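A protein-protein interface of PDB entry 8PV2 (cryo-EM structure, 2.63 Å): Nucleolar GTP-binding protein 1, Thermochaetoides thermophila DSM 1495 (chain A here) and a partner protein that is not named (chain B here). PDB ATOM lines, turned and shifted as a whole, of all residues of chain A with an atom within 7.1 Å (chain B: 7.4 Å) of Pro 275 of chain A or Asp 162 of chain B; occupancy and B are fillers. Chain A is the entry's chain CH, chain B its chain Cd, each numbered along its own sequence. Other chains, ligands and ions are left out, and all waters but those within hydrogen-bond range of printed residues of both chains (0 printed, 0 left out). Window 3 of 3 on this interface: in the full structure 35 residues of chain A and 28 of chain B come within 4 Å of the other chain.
The backbone NH (N) of Asn 159 of chain B is in hydrogen-bond range of the side-chain carboxylate (OE1) of Glu 163 of chain B, at 2.9 Å. N of Glu 163 of chain B sits at hydrogen-bond distance from OG1 of Thr 160 of chain B, at 3.1 Å. The backbone carbonyl oxygen (O) of Leu 164 of chain B is in hydrogen-bond range of the side-chain hydroxyl (OG) of Ser 168 of chain B (3.2 Å). The backbone carbonyl oxygen of Ala 165 of chain B is in hydrogen-bond range of the side-chain hydroxyl of Ser 168 of chain B (2.5 Å).
Among the printed residues, merely in contact across the chains: Leu 228 of chain A with Phe 158 of chain B, Leu 228 of chain A with Asn 159 of chain B, Leu 228 of chain A with Thr 160 of chain B, Leu 228 of chain A with Leu 164 of chain B, Ser 272 of chain A with Val 161 of chain B, Pro 275 of chain A with Val 161 of chain B, Pro 275 of chain A with Asp 162 of chain B, Pro 275 of chain A with Ala 165 of chain B, Leu 276 of chain A with Val 161 of chain B and Leu 276 of chain A with Leu 164 of chain B.
Pro 275 of chain A touches three residues of chain B. Asp 162 of chain B touches one residue of chain A. Printed residues of chain A within 4 Å of Thr 160 of chain B: Leu 228. Of the printed residues of chain B, Leu 228 of chain A touches Phe 158, Asn 159, Thr 160 and Leu 164. Printed residues of chain A within 4 Å of Asn 159 of chain B: Leu 228 (3.9 Å). The nearest residue of chain A that does not touch Asp 162 of chain B is Leu 276 of chain A (6.1 Å).
Hydrophobic or aromatic side chains of chain A within 4 Å of the printed part of chain B: Leu 228, Pro 275 and Leu 276. Among the printed residues, 10 pairs touch across the chains. Among the printed residues, no Asp or Glu carboxylate lies within 4 Å of a Lys or Arg side-chain nitrogen of the other chain.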
ATOM      1  N   LEU A 228     -13.298 -10.171   6.164  1.00  0.00           N
ATOM      2  CA  LEU A 228     -13.473 -11.599   5.909  1.00  0.00           C
ATOM      3  C   LEU A 228     -12.372 -12.163   5.024  1.00  0.00           C
ATOM      4  O   LEU A 228     -12.016 -13.341   5.139  1.00  0.00           O
ATOM      5  CB  LEU A 228     -14.833 -11.852   5.261  1.00  0.00           C
ATOM      6  CG  LEU A 228     -16.083 -11.630   6.105  1.00  0.00           C
ATOM      7  CD1 LEU A 228     -17.306 -12.065   5.327  1.00  0.00           C
ATOM      8  CD2 LEU A 228     -15.994 -12.378   7.414  1.00  0.00           C
ATOM      9  N   PHE A 270     -18.129  -6.989  17.450  1.00  0.00           N
ATOM     10  CA  PHE A 270     -19.566  -7.218  17.586  1.00  0.00           C
ATOM     11  C   PHE A 270     -20.357  -6.382  16.586  1.00  0.00           C
ATOM     12  O   PHE A 270     -21.302  -6.875  15.958  1.00  0.00           O
ATOM     13  CB  PHE A 270     -20.020  -6.912  19.012  1.00  0.00           C
ATOM     14  CG  PHE A 270     -21.482  -7.143  19.230  1.00  0.00           C
ATOM     15  CD1 PHE A 270     -21.967  -8.423  19.410  1.00  0.00           C
ATOM     16  CD2 PHE A 270     -22.373  -6.084  19.245  1.00  0.00           C
ATOM     17  CE1 PHE A 270     -23.308  -8.644  19.600  1.00  0.00           C
ATOM     18  CE2 PHE A 270     -23.721  -6.303  19.434  1.00  0.00           C
ATOM     19  CZ  PHE A 270     -24.187  -7.585  19.614  1.00  0.00           C
ATOM     20  N   LYS A 271     -19.974  -5.114  16.420  1.00  0.00           N
ATOM     21  CA  LYS A 271     -20.646  -4.250  15.452  1.00  0.00           C
ATOM     22  C   LYS A 271     -20.434  -4.742  14.027  1.00  0.00           C
ATOM     23  O   LYS A 271     -21.319  -4.602  13.176  1.00  0.00           O
ATOM     24  CB  LYS A 271     -20.144  -2.816  15.591  1.00  0.00           C
ATOM     25  CG  LYS A 271     -20.561  -2.129  16.869  1.00  0.00           C
ATOM     26  CD  LYS A 271     -19.942  -0.751  16.956  1.00  0.00           C
ATOM     27  CE  LYS A 271     -20.476   0.009  18.149  1.00  0.00           C
ATOM     28  NZ  LYS A 271     -19.784   1.314  18.327  1.00  0.00           N
ATOM     29  N   SER A 272     -19.259  -5.310  13.748  1.00  0.00           N
ATOM     30  CA  SER A 272     -18.979  -5.820  12.411  1.00  0.00           C
ATOM     31  C   SER A 272     -19.815  -7.053  12.095  1.00  0.00           C
ATOM     32  O   SER A 272     -20.293  -7.210  10.966  1.00  0.00           O
ATOM     33  CB  SER A 272     -17.491  -6.134  12.279  1.00  0.00           C
ATOM     34  OG  SER A 272     -16.711  -4.970  12.471  1.00  0.00           O
ATOM     35  N   ILE A 273     -20.008  -7.943  13.076  1.00  0.00           N
ATOM     36  CA  ILE A 273     -20.754  -9.173  12.814  1.00  0.00           C
ATOM     37  C   ILE A 273     -22.236  -9.057  13.150  1.00  0.00           C
ATOM     38  O   ILE A 273     -22.959 -10.055  13.039  1.00  0.00           O
ATOM     39  CB  ILE A 273     -20.173 -10.382  13.571  1.00  0.00           C
ATOM     40  CG1 ILE A 273     -20.274 -10.174  15.081  1.00  0.00           C
ATOM     41  CG2 ILE A 273     -18.742 -10.632  13.137  1.00  0.00           C
ATOM     42  CD1 ILE A 273     -19.531 -11.210  15.894  1.00  0.00           C
ATOM     43  N   LYS A 274     -22.702  -7.883  13.583  1.00  0.00           N
ATOM     44  CA  LYS A 274     -24.141  -7.661  13.736  1.00  0.00           C
ATOM     45  C   LYS A 274     -24.997  -7.924  12.491  1.00  0.00           C
ATOM     46  O   LYS A 274     -26.127  -8.410  12.671  1.00  0.00           O
ATOM     47  CB  LYS A 274     -24.402  -6.242  14.259  1.00  0.00           C
ATOM     48  CG  LYS A 274     -24.464  -6.135  15.768  1.00  0.00           C
ATOM     49  CD  LYS A 274     -24.643  -4.694  16.197  1.00  0.00           C
ATOM     50  CE  LYS A 274     -26.021  -4.183  15.827  1.00  0.00           C
ATOM     51  NZ  LYS A 274     -26.244  -2.801  16.329  1.00  0.00           N
ATOM     52  N   PRO A 275     -24.586  -7.601  11.247  1.00  0.00           N
ATOM     53  CA  PRO A 275     -25.436  -7.977  10.097  1.00  0.00           C
ATOM     54  C   PRO A 275     -25.693  -9.469   9.953  1.00  0.00           C
ATOM     55  O   PRO A 275     -26.700  -9.856   9.345  1.00  0.00           O
ATOM     56  CB  PRO A 275     -24.654  -7.435   8.897  1.00  0.00           C
ATOM     57  CG  PRO A 275     -23.947  -6.284   9.418  1.00  0.00           C
ATOM     58  CD  PRO A 275     -23.549  -6.639  10.817  1.00  0.00           C
ATOM     59  N   LEU A 276     -24.820 -10.322  10.487  1.00  0.00           N
ATOM     60  CA  LEU A 276     -25.088 -11.753  10.509  1.00  0.00           C
ATOM     61  C   LEU A 276     -26.167 -12.131  11.511  1.00  0.00           C
ATOM     62  O   LEU A 276     -26.700 -13.243  11.435  1.00  0.00           O
ATOM     63  CB  LEU A 276     -23.813 -12.525  10.838  1.00  0.00           C
ATOM     64  CG  LEU A 276     -22.707 -12.502   9.792  1.00  0.00           C
ATOM     65  CD1 LEU A 276     -21.519 -13.315  10.266  1.00  0.00           C
ATOM     66  CD2 LEU A 276     -23.223 -13.020   8.470  1.00  0.00           C
ATOM     67  N   PHE A 277     -26.505 -11.238  12.438  1.00  0.00           N
ATOM     68  CA  PHE A 277     -27.391 -11.572  13.545  1.00  0.00           C
ATOM     69  C   PHE A 277     -28.853 -11.287  13.248  1.00  0.00           C
ATOM     70  O   PHE A 277     -29.672 -11.345  14.170  1.00  0.00           O
ATOM     71  CB  PHE A 277     -26.974 -10.808  14.802  1.00  0.00           C
ATOM     72  CG  PHE A 277     -25.634 -11.210  15.343  1.00  0.00           C
ATOM     73  CD1 PHE A 277     -25.090 -12.449  15.045  1.00  0.00           C
ATOM     74  CD2 PHE A 277     -24.919 -10.349  16.155  1.00  0.00           C
ATOM     75  CE1 PHE A 277     -23.857 -12.814  15.536  1.00  0.00           C
ATOM     76  CE2 PHE A 277     -23.687 -10.710  16.655  1.00  0.00           C
ATOM     77  CZ  PHE A 277     -23.157 -11.945  16.345  1.00  0.00           C
ATOM     78  N   ALA A 278     -29.194 -10.959  12.003  1.00  0.00           N
ATOM     79  CA  ALA A 278     -30.585 -10.730  11.641  1.00  0.00           C
ATOM     80  C   ALA A 278     -31.390 -12.017  11.784  1.00  0.00           C
ATOM     81  O   ALA A 278     -30.891 -13.118  11.533  1.00  0.00           O
ATOM     82  CB  ALA A 278     -30.683 -10.203  10.210  1.00  0.00           C
ATOM     83  N   ASN A 279     -32.642 -11.861  12.220  1.00  0.00           N
ATOM     84  CA  ASN A 279     -33.590 -12.929  12.534  1.00  0.00           C
ATOM     85  C   ASN A 279     -33.084 -13.868  13.621  1.00  0.00           C
ATOM     86  O   ASN A 279     -33.520 -15.024  13.683  1.00  0.00           O
ATOM     87  CB  ASN A 279     -33.972 -13.743  11.291  1.00  0.00           C
ATOM     88  CG  ASN A 279     -34.502 -12.876  10.170  1.00  0.00           C
ATOM     89  OD1 ASN A 279     -33.872 -12.747   9.120  1.00  0.00           O
ATOM     90  ND2 ASN A 279     -35.664 -12.273  10.385  1.00  0.00           N
ATOM     91  N   PHE B 158     -18.159 -14.506  -1.317  1.00  0.00           N
ATOM     92  CA  PHE B 158     -18.635 -13.265  -0.731  1.00  0.00           C
ATOM     93  C   PHE B 158     -17.430 -12.500  -0.208  1.00  0.00           C
ATOM     94  O   PHE B 158     -16.381 -13.080   0.077  1.00  0.00           O
ATOM     95  CB  PHE B 158     -19.645 -13.525   0.396  1.00  0.00           C
ATOM     96  CG  PHE B 158     -19.230 -14.620   1.337  1.00  0.00           C
ATOM     97  CD1 PHE B 158     -18.436 -14.341   2.435  1.00  0.00           C
ATOM     98  CD2 PHE B 158     -19.635 -15.927   1.125  1.00  0.00           C
ATOM     99  CE1 PHE B 158     -18.046 -15.343   3.297  1.00  0.00           C
ATOM    100  CE2 PHE B 158     -19.246 -16.932   1.983  1.00  0.00           C
ATOM    101  CZ  PHE B 158     -18.449 -16.640   3.069  1.00  0.00           C
ATOM    102  N   ASN B 159     -17.583 -11.187  -0.086  1.00  0.00           N
ATOM    103  CA  ASN B 159     -16.494 -10.343   0.374  1.00  0.00           C
ATOM    104  C   ASN B 159     -16.814  -9.572   1.646  1.00  0.00           C
ATOM    105  O   ASN B 159     -15.909  -9.356   2.459  1.00  0.00           O
ATOM    106  CB  ASN B 159     -16.089  -9.352  -0.728  1.00  0.00           C
ATOM    107  CG  ASN B 159     -14.618  -8.992  -0.682  1.00  0.00           C
ATOM    108  OD1 ASN B 159     -14.012  -8.927   0.386  1.00  0.00           O
ATOM    109  ND2 ASN B 159     -14.034  -8.759  -1.849  1.00  0.00           N
ATOM    110  N   THR B 160     -18.062  -9.163   1.850  1.00  0.00           N
ATOM    111  CA  THR B 160     -18.446  -8.391   3.019  1.00  0.00           C
ATOM    112  C   THR B 160     -19.449  -9.179   3.850  1.00  0.00           C
ATOM    113  O   THR B 160     -19.990 -10.198   3.415  1.00  0.00           O
ATOM    114  CB  THR B 160     -19.048  -7.034   2.631  1.00  0.00           C
ATOM    115  OG1 THR B 160     -20.391  -7.222   2.171  1.00  0.00           O
ATOM    116  CG2 THR B 160     -18.234  -6.379   1.529  1.00  0.00           C
ATOM    117  N   VAL B 161     -19.692  -8.677   5.061  1.00  0.00           N
ATOM    118  CA  VAL B 161     -20.600  -9.345   5.988  1.00  0.00           C
ATOM    119  C   VAL B 161     -22.039  -9.258   5.487  1.00  0.00           C
ATOM    120  O   VAL B 161     -22.816 -10.214   5.616  1.00  0.00           O
ATOM    121  CB  VAL B 161     -20.435  -8.743   7.397  1.00  0.00           C
ATOM    122  CG1 VAL B 161     -21.431  -9.333   8.368  1.00  0.00           C
ATOM    123  CG2 VAL B 161     -19.020  -8.972   7.895  1.00  0.00           C
ATOM    124  N   ASP B 162     -22.412  -8.120   4.897  1.00  0.00           N
ATOM    125  CA  ASP B 162     -23.754  -7.980   4.339  1.00  0.00           C
ATOM    126  C   ASP B 162     -23.959  -8.905   3.146  1.00  0.00           C
ATOM    127  O   ASP B 162     -25.033  -9.505   2.989  1.00  0.00           O
ATOM    128  CB  ASP B 162     -24.005  -6.527   3.946  1.00  0.00           C
ATOM    129  CG  ASP B 162     -24.120  -5.613   5.148  1.00  0.00           C
ATOM    130  OD1 ASP B 162     -23.194  -4.806   5.374  1.00  0.00           O
ATOM    131  OD2 ASP B 162     -25.136  -5.703   5.867  1.00  0.00           O
ATOM    132  N   GLU B 163     -22.935  -9.035   2.298  1.00  0.00           N
ATOM    133  CA  GLU B 163     -22.994 -10.003   1.209  1.00  0.00           C
ATOM    134  C   GLU B 163     -23.097 -11.426   1.731  1.00  0.00           C
ATOM    135  O   GLU B 163     -23.810 -12.243   1.147  1.00  0.00           O
ATOM    136  CB  GLU B 163     -21.771  -9.871   0.305  1.00  0.00           C
ATOM    137  CG  GLU B 163     -21.728  -8.601  -0.515  1.00  0.00           C
ATOM    138  CD  GLU B 163     -20.401  -8.421  -1.222  1.00  0.00           C
ATOM    139  OE1 GLU B 163     -19.469  -9.203  -0.942  1.00  0.00           O
ATOM    140  OE2 GLU B 163     -20.290  -7.502  -2.059  1.00  0.00           O
ATOM    141  N   LEU B 164     -22.400 -11.738   2.828  1.00  0.00           N
ATOM    142  CA  LEU B 164     -22.504 -13.066   3.426  1.00  0.00           C
ATOM    143  C   LEU B 164     -23.908 -13.334   3.957  1.00  0.00           C
ATOM    144  O   LEU B 164     -24.435 -14.440   3.796  1.00  0.00           O
ATOM    145  CB  LEU B 164     -21.467 -13.213   4.537  1.00  0.00           C
ATOM    146  CG  LEU B 164     -21.488 -14.459   5.425  1.00  0.00           C
ATOM    147  CD1 LEU B 164     -21.505 -15.743   4.620  1.00  0.00           C
ATOM    148  CD2 LEU B 164     -20.289 -14.433   6.343  1.00  0.00           C
ATOM    149  N   ALA B 165     -24.525 -12.337   4.594  1.00  0.00           N
ATOM    150  CA  ALA B 165     -25.885 -12.510   5.103  1.00  0.00           C
ATOM    151  C   ALA B 165     -26.880 -12.727   3.968  1.00  0.00           C
ATOM    152  O   ALA B 165     -27.724 -13.638   4.030  1.00  0.00           O
ATOM    153  CB  ALA B 165     -26.283 -11.302   5.947  1.00  0.00           C
ATOM    154  N   GLY B 166     -26.777 -11.919   2.909  1.00  0.00           N
ATOM    155  CA  GLY B 166     -27.640 -12.119   1.754  1.00  0.00           C
ATOM    156  C   GLY B 166     -27.411 -13.456   1.074  1.00  0.00           C
ATOM    157  O   GLY B 166     -28.362 -14.120   0.649  1.00  0.00           O
ATOM    158  N   TYR B 167     -26.146 -13.876   0.983  1.00  0.00           N
ATOM    159  CA  TYR B 167     -25.812 -15.153   0.369  1.00  0.00           C
ATOM    160  C   TYR B 167     -26.370 -16.312   1.174  1.00  0.00           C
ATOM    161  O   TYR B 167     -26.840 -17.300   0.604  1.00  0.00           O
ATOM    162  CB  TYR B 167     -24.294 -15.271   0.226  1.00  0.00           C
ATOM    163  CG  TYR B 167     -23.795 -16.670  -0.042  1.00  0.00           C
ATOM    164  CD1 TYR B 167     -23.952 -17.250  -1.291  1.00  0.00           C
ATOM    165  CD2 TYR B 167     -23.154 -17.404   0.947  1.00  0.00           C
ATOM    166  CE1 TYR B 167     -23.496 -18.526  -1.548  1.00  0.00           C
ATOM    167  CE2 TYR B 167     -22.696 -18.683   0.700  1.00  0.00           C
ATOM    168  CZ  TYR B 167     -22.870 -19.236  -0.550  1.00  0.00           C
ATOM    169  OH  TYR B 167     -22.415 -20.505  -0.809  1.00  0.00           O
ATOM    170  N   SER B 168     -26.330 -16.208   2.504  1.00  0.00           N
ATOM    171  CA  SER B 168     -26.907 -17.247   3.352  1.00  0.00           C
ATOM    172  C   SER B 168     -28.418 -17.322   3.173  1.00  0.00           C
ATOM    173  O   SER B 168     -28.996 -18.417   3.150  1.00  0.00           O
ATOM    174  CB  SER B 168     -26.545 -16.990   4.812  1.00  0.00           C
ATOM    175  OG  SER B 168     -27.027 -15.730   5.237  1.00  0.00           O
